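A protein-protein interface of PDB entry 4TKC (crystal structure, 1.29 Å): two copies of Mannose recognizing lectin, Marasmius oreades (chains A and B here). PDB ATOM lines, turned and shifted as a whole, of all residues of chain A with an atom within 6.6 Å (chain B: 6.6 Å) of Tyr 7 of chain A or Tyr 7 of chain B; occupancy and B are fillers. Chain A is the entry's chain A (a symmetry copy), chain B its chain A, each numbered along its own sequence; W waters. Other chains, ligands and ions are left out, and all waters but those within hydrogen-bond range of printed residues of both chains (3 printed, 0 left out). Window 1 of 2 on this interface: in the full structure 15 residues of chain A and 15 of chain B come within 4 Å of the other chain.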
ATOM      1  N   VAL A   4       3.757 -27.500  26.758  1.00  0.00           N
ATOM      2  CA  VAL A   4       4.525 -26.778  25.765  1.00  0.00           C
ATOM      3  C   VAL A   4       5.879 -27.483  25.487  1.00  0.00           C
ATOM      4  O   VAL A   4       6.526 -27.973  26.393  1.00  0.00           O
ATOM      5  CB  VAL A   4       4.686 -25.308  26.181  1.00  0.00           C
ATOM      6  CG1 VAL A   4       5.589 -24.595  25.209  1.00  0.00           C
ATOM      7  CG2 VAL A   4       3.329 -24.647  26.246  1.00  0.00           C
ATOM      8  N   HIS A   5       6.315 -27.441  24.229  1.00  0.00           N
ATOM      9  CA  HIS A   5       7.524 -28.119  23.783  1.00  0.00           C
ATOM     10  C   HIS A   5       8.589 -27.137  23.276  1.00  0.00           C
ATOM     11  O   HIS A   5       8.579 -26.777  22.101  1.00  0.00           O
ATOM     12  CB  HIS A   5       7.143 -29.094  22.684  1.00  0.00           C
ATOM     13  CG  HIS A   5       6.102 -30.071  23.114  1.00  0.00           C
ATOM     14  ND1 HIS A   5       4.995 -30.372  22.343  1.00  0.00           N
ATOM     15  CD2 HIS A   5       5.953 -30.749  24.275  1.00  0.00           C
ATOM     16  CE1 HIS A   5       4.253 -31.260  22.983  1.00  0.00           C
ATOM     17  NE2 HIS A   5       4.830 -31.534  24.141  1.00  0.00           N
ATOM     18  N   PRO A   6       9.518 -26.716  24.178  1.00  0.00           N
ATOM     19  CA  PRO A   6      10.480 -25.673  23.768  1.00  0.00           C
ATOM     20  C   PRO A   6      11.687 -26.240  23.058  1.00  0.00           C
ATOM     21  O   PRO A   6      12.550 -25.498  22.603  1.00  0.00           O
ATOM     22  CB  PRO A   6      10.918 -25.053  25.088  1.00  0.00           C
ATOM     23  CG  PRO A   6      10.027 -25.581  26.145  1.00  0.00           C
ATOM     24  CD  PRO A   6       9.494 -26.891  25.633  1.00  0.00           C
ATOM     25  N   TYR A   7      11.734 -27.582  22.967  1.00  0.00           N
ATOM     26  CA  TYR A   7      12.960 -28.277  22.585  1.00  0.00           C
ATOM     27  C   TYR A   7      12.762 -29.387  21.551  1.00  0.00           C
ATOM     28  O   TYR A   7      13.724 -30.123  21.271  1.00  0.00           O
ATOM     29  CB  TYR A   7      13.600 -28.907  23.837  1.00  0.00           C
ATOM     30  CG  TYR A   7      14.231 -27.934  24.772  1.00  0.00           C
ATOM     31  CD1 TYR A   7      15.475 -27.451  24.477  1.00  0.00           C
ATOM     32  CD2 TYR A   7      13.720 -27.744  26.026  1.00  0.00           C
ATOM     33  CE1 TYR A   7      16.060 -26.524  25.317  1.00  0.00           C
ATOM     34  CE2 TYR A   7      14.306 -26.828  26.894  1.00  0.00           C
ATOM     35  CZ  TYR A   7      15.526 -26.295  26.558  1.00  0.00           C
ATOM     36  OH  TYR A   7      16.138 -25.412  27.475  1.00  0.00           O
ATOM     37  N   GLY A   8      11.557 -29.526  21.002  1.00  0.00           N
ATOM     38  CA  GLY A   8      11.249 -30.742  20.209  1.00  0.00           C
ATOM     39  C   GLY A   8      11.499 -32.001  21.055  1.00  0.00           C
ATOM     40  O   GLY A   8      11.056 -32.118  22.188  1.00  0.00           O
ATOM     41  N   SER A   9      12.326 -32.888  20.503  1.00  0.00           N
ATOM     42  CA  SER A   9      12.616 -34.160  21.171  1.00  0.00           C
ATOM     43  C   SER A   9      13.770 -34.190  22.161  1.00  0.00           C
ATOM     44  O   SER A   9      13.940 -35.125  22.945  1.00  0.00           O
ATOM     45  CB  SER A   9      12.967 -35.225  20.104  1.00  0.00           C
ATOM     46  OG  SER A   9      14.210 -34.900  19.464  1.00  0.00           O
ATOM     47  N   THR A  10      14.576 -33.123  22.159  1.00  0.00           N
ATOM     48  CA  THR A  10      15.905 -33.242  22.701  1.00  0.00           C
ATOM     49  C   THR A  10      16.297 -32.109  23.660  1.00  0.00           C
ATOM     50  O   THR A  10      16.171 -30.919  23.315  1.00  0.00           O
ATOM     51  CB  THR A  10      16.930 -33.343  21.548  1.00  0.00           C
ATOM     52  OG1 THR A  10      16.631 -34.490  20.721  1.00  0.00           O
ATOM     53  CG2 THR A  10      18.386 -33.401  22.058  1.00  0.00           C
ATOM     54  N   LEU A  11      16.727 -32.475  24.862  1.00  0.00           N
ATOM     55  CA  LEU A  11      17.236 -31.544  25.871  1.00  0.00           C
ATOM     56  C   LEU A  11      18.748 -31.532  25.797  1.00  0.00           C
ATOM     57  O   LEU A  11      19.394 -32.482  26.198  1.00  0.00           O
ATOM     58  CB  LEU A  11      16.794 -31.984  27.281  1.00  0.00           C
ATOM     59  CG  LEU A  11      16.785 -30.876  28.321  1.00  0.00           C
ATOM     60  CD1 LEU A  11      15.817 -29.758  27.929  1.00  0.00           C
ATOM     61  CD2 LEU A  11      16.440 -31.415  29.688  1.00  0.00           C
ATOM     62  N   PRO A  12      19.335 -30.511  25.176  1.00  0.00           N
ATOM     63  CA  PRO A  12      20.796 -30.391  25.136  1.00  0.00           C
ATOM     64  C   PRO A  12      21.394 -29.861  26.457  1.00  0.00           C
ATOM     65  O   PRO A  12      20.654 -29.583  27.394  1.00  0.00           O
ATOM     66  CB  PRO A  12      21.030 -29.383  23.997  1.00  0.00           C
ATOM     67  CG  PRO A  12      19.748 -28.662  23.828  1.00  0.00           C
ATOM     68  CD  PRO A  12      18.665 -29.327  24.605  1.00  0.00           C
ATOM     69  N   ASN A  14      22.637 -27.575  29.202  1.00  0.00           N
ATOM     70  CA  ASN A  14      21.991 -26.329  29.698  1.00  0.00           C
ATOM     71  C   ASN A  14      20.507 -26.254  29.420  1.00  0.00           C
ATOM     72  O   ASN A  14      19.854 -25.263  29.693  1.00  0.00           O
ATOM     73  CB  ASN A  14      22.658 -25.036  29.184  1.00  0.00           C
ATOM     74  CG  ASN A  14      24.023 -24.847  29.773  1.00  0.00           C
ATOM     75  OD1 ASN A  14      24.199 -25.001  30.997  1.00  0.00           O
ATOM     76  ND2 ASN A  14      25.015 -24.650  28.919  1.00  0.00           N
ATOM     77  N   GLY A  15      19.941 -27.316  28.872  1.00  0.00           N
ATOM     78  CA  GLY A  15      18.524 -27.352  28.663  1.00  0.00           C
ATOM     79  C   GLY A  15      17.758 -27.605  29.957  1.00  0.00           C
ATOM     80  O   GLY A  15      18.107 -28.518  30.719  1.00  0.00           O
ATOM     81  N   VAL A  16      16.582 -26.983  30.084  1.00  0.00           N
ATOM     82  CA  VAL A  16      15.746 -27.148  31.240  1.00  0.00           C
ATOM     83  C   VAL A  16      14.289 -27.258  30.849  1.00  0.00           C
ATOM     84  O   VAL A  16      13.773 -26.473  30.050  1.00  0.00           O
ATOM     85  CB  VAL A  16      15.860 -25.939  32.212  1.00  0.00           C
ATOM     86  CG1 VAL A  16      14.756 -26.016  33.261  1.00  0.00           C
ATOM     87  CG2 VAL A  16      17.211 -25.974  32.883  1.00  0.00           C
ATOM     88  N   ILE A  17      13.648 -28.309  31.394  1.00  0.00           N
ATOM     89  CA  ILE A  17      12.187 -28.466  31.314  1.00  0.00           C
ATOM     90  C   ILE A  17      11.527 -28.180  32.653  1.00  0.00           C
ATOM     91  O   ILE A  17      11.837 -28.849  33.641  1.00  0.00           O
ATOM     92  CB  ILE A  17      11.742 -29.934  31.064  1.00  0.00           C
ATOM     93  CG1 ILE A  17      12.591 -30.647  30.047  1.00  0.00           C
ATOM     94  CG2 ILE A  17      10.272 -29.982  30.695  1.00  0.00           C
ATOM     95  CD1 ILE A  17      12.183 -32.092  29.880  1.00  0.00           C
ATOM     96  N   ALA A  22       7.590 -30.059  28.250  1.00  0.00           N
ATOM     97  CA  ALA A  22       7.879 -31.481  27.908  1.00  0.00           C
ATOM     98  C   ALA A  22       8.768 -31.580  26.691  1.00  0.00           C
ATOM     99  O   ALA A  22       8.739 -30.681  25.825  1.00  0.00           O
ATOM    100  CB  ALA A  22       6.587 -32.258  27.688  1.00  0.00           C
ATOM    101  N   LEU A  23       9.494 -32.707  26.567  1.00  0.00           N
ATOM    102  CA  LEU A  23      10.031 -33.124  25.275  1.00  0.00           C
ATOM    103  C   LEU A  23       8.916 -33.923  24.582  1.00  0.00           C
ATOM    104  O   LEU A  23       8.123 -34.572  25.258  1.00  0.00           O
ATOM    105  CB  LEU A  23      11.241 -34.073  25.412  1.00  0.00           C
ATOM    106  CG  LEU A  23      12.376 -33.527  26.282  1.00  0.00           C
ATOM    107  CD1 LEU A  23      13.557 -34.472  26.427  1.00  0.00           C
ATOM    108  CD2 LEU A  23      12.828 -32.202  25.693  1.00  0.00           C
ATOM    109  N   ILE A  24       8.920 -33.871  23.255  1.00  0.00           N
ATOM    110  CA  ILE A  24       7.965 -34.628  22.436  1.00  0.00           C
ATOM    111  C   ILE A  24       8.713 -35.313  21.300  1.00  0.00           C
ATOM    112  O   ILE A  24       9.616 -34.775  20.697  1.00  0.00           O
ATOM    113  CB  ILE A  24       6.842 -33.679  21.894  1.00  0.00           C
ATOM    114  CG1 ILE A  24       5.698 -34.433  21.201  1.00  0.00           C
ATOM    115  CG2 ILE A  24       7.421 -32.588  20.997  1.00  0.00           C
ATOM    116  CD1 ILE A  24       4.875 -35.262  22.154  1.00  0.00           C
ATOM    117  N   PHE A  60      11.917 -28.953  38.002  1.00  0.00           N
ATOM    118  CA  PHE A  60      12.484 -28.920  36.663  1.00  0.00           C
ATOM    119  C   PHE A  60      13.476 -30.090  36.480  1.00  0.00           C
ATOM    120  O   PHE A  60      14.012 -30.593  37.460  1.00  0.00           O
ATOM    121  CB  PHE A  60      13.116 -27.520  36.341  1.00  0.00           C
ATOM    122  CG  PHE A  60      14.296 -27.173  37.193  1.00  0.00           C
ATOM    123  CD1 PHE A  60      14.117 -26.425  38.349  1.00  0.00           C
ATOM    124  CD2 PHE A  60      15.594 -27.430  36.767  1.00  0.00           C
ATOM    125  CE1 PHE A  60      15.194 -26.062  39.126  1.00  0.00           C
ATOM    126  CE2 PHE A  60      16.679 -27.057  37.557  1.00  0.00           C
ATOM    127  CZ  PHE A  60      16.468 -26.380  38.740  1.00  0.00           C
ATOM    128  N   LYS A  62      17.151 -30.724  34.263  1.00  0.00           N
ATOM    129  CA  LYS A  62      18.215 -30.038  33.567  1.00  0.00           C
ATOM    130  C   LYS A  62      19.222 -31.080  33.078  1.00  0.00           C
ATOM    131  O   LYS A  62      19.773 -31.849  33.890  1.00  0.00           O
ATOM    132  CB  LYS A  62      18.885 -29.015  34.516  1.00  0.00           C
ATOM    133  CG  LYS A  62      19.990 -28.186  33.851  1.00  0.00           C
ATOM    134  CD  LYS A  62      20.315 -26.975  34.711  1.00  0.00           C
ATOM    135  CE  LYS A  62      21.166 -25.943  33.992  1.00  0.00           C
ATOM    136  NZ  LYS A  62      21.636 -24.809  34.850  1.00  0.00           N
ATOM    137  N   VAL B   4      11.219 -19.982  40.536  1.00  0.00           N
ATOM    138  CA  VAL B   4      12.350 -20.884  40.599  1.00  0.00           C
ATOM    139  C   VAL B   4      13.490 -20.416  39.656  1.00  0.00           C
ATOM    140  O   VAL B   4      13.243 -19.964  38.553  1.00  0.00           O
ATOM    141  CB  VAL B   4      11.897 -22.326  40.325  1.00  0.00           C
ATOM    142  CG1 VAL B   4      13.094 -23.239  40.270  1.00  0.00           C
ATOM    143  CG2 VAL B   4      10.929 -22.766  41.400  1.00  0.00           C
ATOM    144  N   HIS B   5      14.733 -20.618  40.092  1.00  0.00           N
ATOM    145  CA  HIS B   5      15.912 -20.167  39.368  1.00  0.00           C
ATOM    146  C   HIS B   5      16.801 -21.335  38.918  1.00  0.00           C
ATOM    147  O   HIS B   5      17.662 -21.775  39.676  1.00  0.00           O
ATOM    148  CB  HIS B   5      16.693 -19.229  40.271  1.00  0.00           C
ATOM    149  CG  HIS B   5      15.879 -18.076  40.750  1.00  0.00           C
ATOM    150  ND1 HIS B   5      15.864 -17.669  42.069  1.00  0.00           N
ATOM    151  CD2 HIS B   5      14.982 -17.299  40.101  1.00  0.00           C
ATOM    152  CE1 HIS B   5      15.051 -16.633  42.191  1.00  0.00           C
ATOM    153  NE2 HIS B   5      14.531 -16.364  41.006  1.00  0.00           N
ATOM    154  N   PRO B   6      16.588 -21.823  37.665  1.00  0.00           N
ATOM    155  CA  PRO B   6      17.329 -23.028  37.241  1.00  0.00           C
ATOM    156  C   PRO B   6      18.699 -22.706  36.689  1.00  0.00           C
ATOM    157  O   PRO B   6      19.462 -23.603  36.348  1.00  0.00           O
ATOM    158  CB  PRO B   6      16.463 -23.608  36.131  1.00  0.00           C
ATOM    159  CG  PRO B   6      15.179 -22.873  36.140  1.00  0.00           C
ATOM    160  CD  PRO B   6      15.461 -21.539  36.774  1.00  0.00           C
ATOM    161  N   TYR B   7      19.003 -21.398  36.608  1.00  0.00           N
ATOM    162  CA  TYR B   7      20.145 -20.927  35.830  1.00  0.00           C
ATOM    163  C   TYR B   7      21.006 -19.881  36.540  1.00  0.00           C
ATOM    164  O   TYR B   7      21.916 -19.322  35.902  1.00  0.00           O
ATOM    165  CB  TYR B   7      19.644 -20.310  34.511  1.00  0.00           C
ATOM    166  CG  TYR B   7      19.142 -21.296  33.512  1.00  0.00           C
ATOM    167  CD1 TYR B   7      20.049 -21.983  32.755  1.00  0.00           C
ATOM    168  CD2 TYR B   7      17.823 -21.312  33.155  1.00  0.00           C
ATOM    169  CE1 TYR B   7      19.600 -22.923  31.847  1.00  0.00           C
ATOM    170  CE2 TYR B   7      17.355 -22.239  32.229  1.00  0.00           C
ATOM    171  CZ  TYR B   7      18.271 -22.975  31.518  1.00  0.00           C
ATOM    172  OH  TYR B   7      17.786 -23.870  30.539  1.00  0.00           O
ATOM    173  N   GLY B   8      20.734 -19.601  37.812  1.00  0.00           N
ATOM    174  CA  GLY B   8      21.354 -18.415  38.452  1.00  0.00           C
ATOM    175  C   GLY B   8      21.034 -17.149  37.641  1.00  0.00           C
ATOM    176  O   GLY B   8      19.896 -16.882  37.282  1.00  0.00           O
ATOM    177  N   SER B   9      22.099 -16.442  37.266  1.00  0.00           N
ATOM    178  CA  SER B   9      21.943 -15.182  36.532  1.00  0.00           C
ATOM    179  C   SER B   9      21.865 -15.255  35.015  1.00  0.00           C
ATOM    180  O   SER B   9      21.494 -14.301  34.329  1.00  0.00           O
ATOM    181  CB  SER B   9      23.153 -14.265  36.835  1.00  0.00           C
ATOM    182  OG  SER B   9      24.353 -14.823  36.278  1.00  0.00           O
ATOM    183  N   THR B  10      22.188 -16.429  34.464  1.00  0.00           N
ATOM    184  CA  THR B  10      22.581 -16.474  33.078  1.00  0.00           C
ATOM    185  C   THR B  10      21.892 -17.579  32.265  1.00  0.00           C
ATOM    186  O   THR B  10      21.906 -18.758  32.666  1.00  0.00           O
ATOM    187  CB  THR B  10      24.117 -16.616  32.978  1.00  0.00           C
ATOM    188  OG1 THR B  10      24.760 -15.501  33.636  1.00  0.00           O
ATOM    189  CG2 THR B  10      24.601 -16.743  31.517  1.00  0.00           C
ATOM    190  N   LEU B  11      21.263 -17.194  31.160  1.00  0.00           N
ATOM    191  CA  LEU B  11      20.636 -18.114  30.209  1.00  0.00           C
ATOM    192  C   LEU B  11      21.603 -18.361  29.070  1.00  0.00           C
ATOM    193  O   LEU B  11      21.821 -17.493  28.245  1.00  0.00           O
ATOM    194  CB  LEU B  11      19.333 -17.508  29.654  1.00  0.00           C
ATOM    195  CG  LEU B  11      18.342 -18.521  29.104  1.00  0.00           C
ATOM    196  CD1 LEU B  11      17.898 -19.504  30.187  1.00  0.00           C
ATOM    197  CD2 LEU B  11      17.145 -17.835  28.493  1.00  0.00           C
ATOM    198  N   PRO B  12      22.287 -19.502  29.068  1.00  0.00           N
ATOM    199  CA  PRO B  12      23.179 -19.846  27.956  1.00  0.00           C
ATOM    200  C   PRO B  12      22.421 -20.361  26.712  1.00  0.00           C
ATOM    201  O   PRO B  12      21.199 -20.453  26.737  1.00  0.00           O
ATOM    202  CB  PRO B  12      24.059 -20.961  28.548  1.00  0.00           C
ATOM    203  CG  PRO B  12      23.312 -21.489  29.712  1.00  0.00           C
ATOM    204  CD  PRO B  12      22.152 -20.610  30.033  1.00  0.00           C
ATOM    205  N   ASN B  14      20.669 -22.599  24.217  1.00  0.00           N
ATOM    206  CA  ASN B  14      19.701 -23.691  24.512  1.00  0.00           C
ATOM    207  C   ASN B  14      19.015 -23.560  25.852  1.00  0.00           C
ATOM    208  O   ASN B  14      18.258 -24.417  26.270  1.00  0.00           O
ATOM    209  CB  ASN B  14      20.309 -25.105  24.401  1.00  0.00           C
ATOM    210  CG  ASN B  14      20.639 -25.456  22.982  1.00  0.00           C
ATOM    211  OD1 ASN B  14      19.808 -25.239  22.079  1.00  0.00           O
ATOM    212  ND2 ASN B  14      21.876 -25.864  22.744  1.00  0.00           N
ATOM    213  N   GLY B  15      19.267 -22.468  26.554  1.00  0.00           N
ATOM    214  CA  GLY B  15      18.583 -22.233  27.792  1.00  0.00           C
ATOM    215  C   GLY B  15      17.147 -21.771  27.577  1.00  0.00           C
ATOM    216  O   GLY B  15      16.898 -20.867  26.767  1.00  0.00           O
ATOM    217  N   VAL B  16      16.246 -22.195  28.467  1.00  0.00           N
ATOM    218  CA  VAL B  16      14.861 -21.819  28.398  1.00  0.00           C
ATOM    219  C   VAL B  16      14.308 -21.518  29.773  1.00  0.00           C
ATOM    220  O   VAL B  16      14.505 -22.272  30.730  1.00  0.00           O
ATOM    221  CB  VAL B  16      13.983 -22.955  27.801  1.00  0.00           C
ATOM    222  CG1 VAL B  16      12.508 -22.633  28.015  1.00  0.00           C
ATOM    223  CG2 VAL B  16      14.275 -23.077  26.325  1.00  0.00           C
ATOM    224  N   ILE B  17      13.655 -20.344  29.863  1.00  0.00           N
ATOM    225  CA  ILE B  17      12.863 -19.973  31.047  1.00  0.00           C
ATOM    226  C   ILE B  17      11.372 -20.054  30.761  1.00  0.00           C
ATOM    227  O   ILE B  17      10.886 -19.369  29.859  1.00  0.00           O
ATOM    228  CB  ILE B  17      13.015 -18.477  31.441  1.00  0.00           C
ATOM    229  CG1 ILE B  17      14.431 -17.980  31.347  1.00  0.00           C
ATOM    230  CG2 ILE B  17      12.427 -18.234  32.817  1.00  0.00           C
ATOM    231  CD1 ILE B  17      14.538 -16.505  31.662  1.00  0.00           C
ATOM    232  N   ALA B  22      12.743 -17.932  36.420  1.00  0.00           N
ATOM    233  CA  ALA B  22      13.402 -16.599  36.299  1.00  0.00           C
ATOM    234  C   ALA B  22      14.907 -16.728  36.343  1.00  0.00           C
ATOM    235  O   ALA B  22      15.432 -17.674  36.966  1.00  0.00           O
ATOM    236  CB  ALA B  22      12.916 -15.654  37.389  1.00  0.00           C
ATOM    237  N   LEU B  23      15.612 -15.738  35.767  1.00  0.00           N
ATOM    238  CA  LEU B  23      17.011 -15.504  36.109  1.00  0.00           C
ATOM    239  C   LEU B  23      17.006 -14.599  37.352  1.00  0.00           C
ATOM    240  O   LEU B  23      16.097 -13.788  37.508  1.00  0.00           O
ATOM    241  CB  LEU B  23      17.776 -14.743  35.006  1.00  0.00           C
ATOM    242  CG  LEU B  23      17.693 -15.388  33.620  1.00  0.00           C
ATOM    243  CD1 LEU B  23      18.434 -14.626  32.534  1.00  0.00           C
ATOM    244  CD2 LEU B  23      18.225 -16.807  33.727  1.00  0.00           C
ATOM    245  N   ILE B  24      18.042 -14.749  38.169  1.00  0.00           N
ATOM    246  CA  ILE B  24      18.224 -13.919  39.366  1.00  0.00           C
ATOM    247  C   ILE B  24      19.669 -13.443  39.428  1.00  0.00           C
ATOM    248  O   ILE B  24      20.604 -14.156  39.131  1.00  0.00           O
ATOM    249  CB  ILE B  24      17.830 -14.724  40.652  1.00  0.00           C
ATOM    250  CG1 ILE B  24      17.800 -13.858  41.919  1.00  0.00           C
ATOM    251  CG2 ILE B  24      18.717 -15.955  40.831  1.00  0.00           C
ATOM    252  CD1 ILE B  24      16.684 -12.845  41.916  1.00  0.00           C
ATOM    253  N   PHE B  60       7.530 -18.954  27.103  1.00  0.00           N
ATOM    254  CA  PHE B  60       8.916 -19.172  27.486  1.00  0.00           C
ATOM    255  C   PHE B  60       9.833 -18.184  26.733  1.00  0.00           C
ATOM    256  O   PHE B  60       9.464 -17.697  25.671  1.00  0.00           O
ATOM    257  CB  PHE B  60       9.335 -20.672  27.293  1.00  0.00           C
ATOM    258  CG  PHE B  60       9.323 -21.130  25.868  1.00  0.00           C
ATOM    259  CD1 PHE B  60       8.195 -21.753  25.352  1.00  0.00           C
ATOM    260  CD2 PHE B  60      10.477 -21.106  25.093  1.00  0.00           C
ATOM    261  CE1 PHE B  60       8.179 -22.218  24.056  1.00  0.00           C
ATOM    262  CE2 PHE B  60      10.454 -21.580  23.784  1.00  0.00           C
ATOM    263  CZ  PHE B  60       9.296 -22.127  23.271  1.00  0.00           C
ATOM    264  N   LYS B  62      13.879 -18.283  25.169  1.00  0.00           N
ATOM    265  CA  LYS B  62      14.960 -19.173  24.814  1.00  0.00           C
ATOM    266  C   LYS B  62      16.107 -18.335  24.248  1.00  0.00           C
ATOM    267  O   LYS B  62      15.920 -17.601  23.258  1.00  0.00           O
ATOM    268  CB  LYS B  62      14.463 -20.212  23.780  1.00  0.00           C
ATOM    269  CG  LYS B  62      15.523 -21.247  23.385  1.00  0.00           C
ATOM    270  CD  LYS B  62      14.860 -22.426  22.690  1.00  0.00           C
ATOM    271  CE  LYS B  62      15.778 -23.626  22.543  1.00  0.00           C
ATOM    272  NZ  LYS B  62      15.216 -24.752  21.730  1.00  0.00           N
HETATM  273  O   HOH W   1      22.823 -22.507  36.799  1.00  0.00           O
HETATM  274  O   HOH W   2      14.051 -27.055  19.771  1.00  0.00           O
HETATM  275  O   HOH W   3      12.782 -24.245  31.054  1.00  0.00           O
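Val 4 of chain A touches Phe 60 of chain B (CG1 to CE1, 3.7 Å). OH of Tyr 7 of chain A touches OH of Tyr 7 of chain B, at 3.8 Å. C of Gly 15 of chain B touches OH of Tyr 7 of chain A, 3.8 Å away. Tyr 7 of chain A touches Lys 62 of chain B. Asn 14 of chain A touches Asn 14 of chain B (O to O, 3.9 Å). Asn 14 of chain A touches Gly 15 of chain B (O to CA, 3.8 Å). O of Asn 14 of chain B touches CA of Gly 15 of chain A (3.8 Å). CG1 of Val 4 of chain B touches CE1 of Phe 60 of chain A (3.7 Å). CB of Pro 6 of chain B touches CE2 of Phe 60 of chain A, at 3.7 Å. NZ of Lys 62 of chain A touches CD1 of Tyr 7 of chain B (3.9 Å).
Hydrophobic or aromatic side chains of chain A that line the printed part of chain B: Val 4, Pro 6, Tyr 7, Pro 12, Val 16 and Phe 60. Hydrophobic or aromatic side chains of chain B that line the printed part of chain A: Val 4, Pro 6, Tyr 7, Pro 12, Val 16 and Phe 60. Along chain B the printed residues that touch a printed residue of chain A span positions 4 to 62. Among the printed residues, 20 pairs touch across the chains. Among the printed residues, no Asp or Glu carboxylate lies within 4 Å of a Lys or Arg side-chain nitrogen of the other chain.
Water W3 bridges O of Val 16 of chain A (2.6 Å) and O of Val 16 of chain B (2.6 Å). Water W2 lies within hydrogen-bond range of the side-chain amino group of Lys 62 of chain B (3.2 Å) and the backbone carbonyl oxygen of Tyr 7 of chain A (3.4 Å). Water W1 bridges the side-chain amino group (NZ) of Lys 62 of chain A and the backbone carbonyl oxygen (O) of Tyr 7 of chain B.
The backbone NH of Val 16 of chain B is in hydrogen-bond range of the side-chain hydroxyl of Tyr 7 of chain B (3.1 Å). The backbone carbonyl oxygen (O) of Val 4 of chain A is in hydrogen-bond range of the backbone NH (N) of Ala 22 of chain A (3.0 Å). N of Val 16 of chain A lies within hydrogen-bond range of OH of Tyr 7 of chain A (3.1 Å). N of Ala 22 of chain B lies within hydrogen-bond range of O of Val 4 of chain B, 3.0 Å away.
The backbone carbonyl oxygen (O) of Asn 14 of chain B is in hydrogen-bond range of the side-chain hydroxyl (OH) of Tyr 7 of chain A (2.6 Å). NZ of Lys 62 of chain A is in hydrogen-bond range of O of Pro 6 of chain B, 2.9 Å away. The side-chain amino group (NZ) of Lys 62 of chain B lies within hydrogen-bond range of the backbone carbonyl oxygen (O) of Pro 6 of chain A. OH of Tyr 7 of chain B sits at hydrogen-bond distance from O of Asn 14 of chain A (2.6 Å). N of Val 16 of chain B sits close to OH of Tyr 7 of chain A (3.4 Å). N of Val 16 of chain A sits close to OH of Tyr 7 of chain B, 3.4 Å away.
Tyr 7 of chain A touches five residues of chain B. His 5 of chain B touches none of the printed residues of chain A. Tyr 7 of chain B touches five residues of chain A. Printed residues of chain A within 4 Å of Pro 12 of chain B: Asn 14. Of the printed residues of chain A, Asn 14 of chain B touches Tyr 7, Pro 12, Asn 14 and Gly 15. Of the printed residues of chain A, Gly 15 of chain B touches Tyr 7 (3.8 Å) and Asn 14 (3.8 Å). The nearest residue of chain B that does not touch Tyr 7 of chain A is Phe 60 of chain B (6.0 Å). The nearest residue of chain A that does not touch Tyr 7 of chain B is Phe 60 of chain A (6.0 Å).
Pro 6 of chain A touches Lys 62 of chain B, and with the chains exchanged Lys 62 of chain A touches Pro 6 of chain B. Tyr 7 of chain A touches Gly 15 of chain B, and with the chains exchanged Gly 15 of chain A touches Tyr 7 of chain B. Tyr 7 of chain A touches Lys 62 of chain B, and with the chains exchanged Lys 62 of chain A touches Tyr 7 of chain B. Asn 14 of chain A touches its own counterpart, Asn 14 of chain B.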
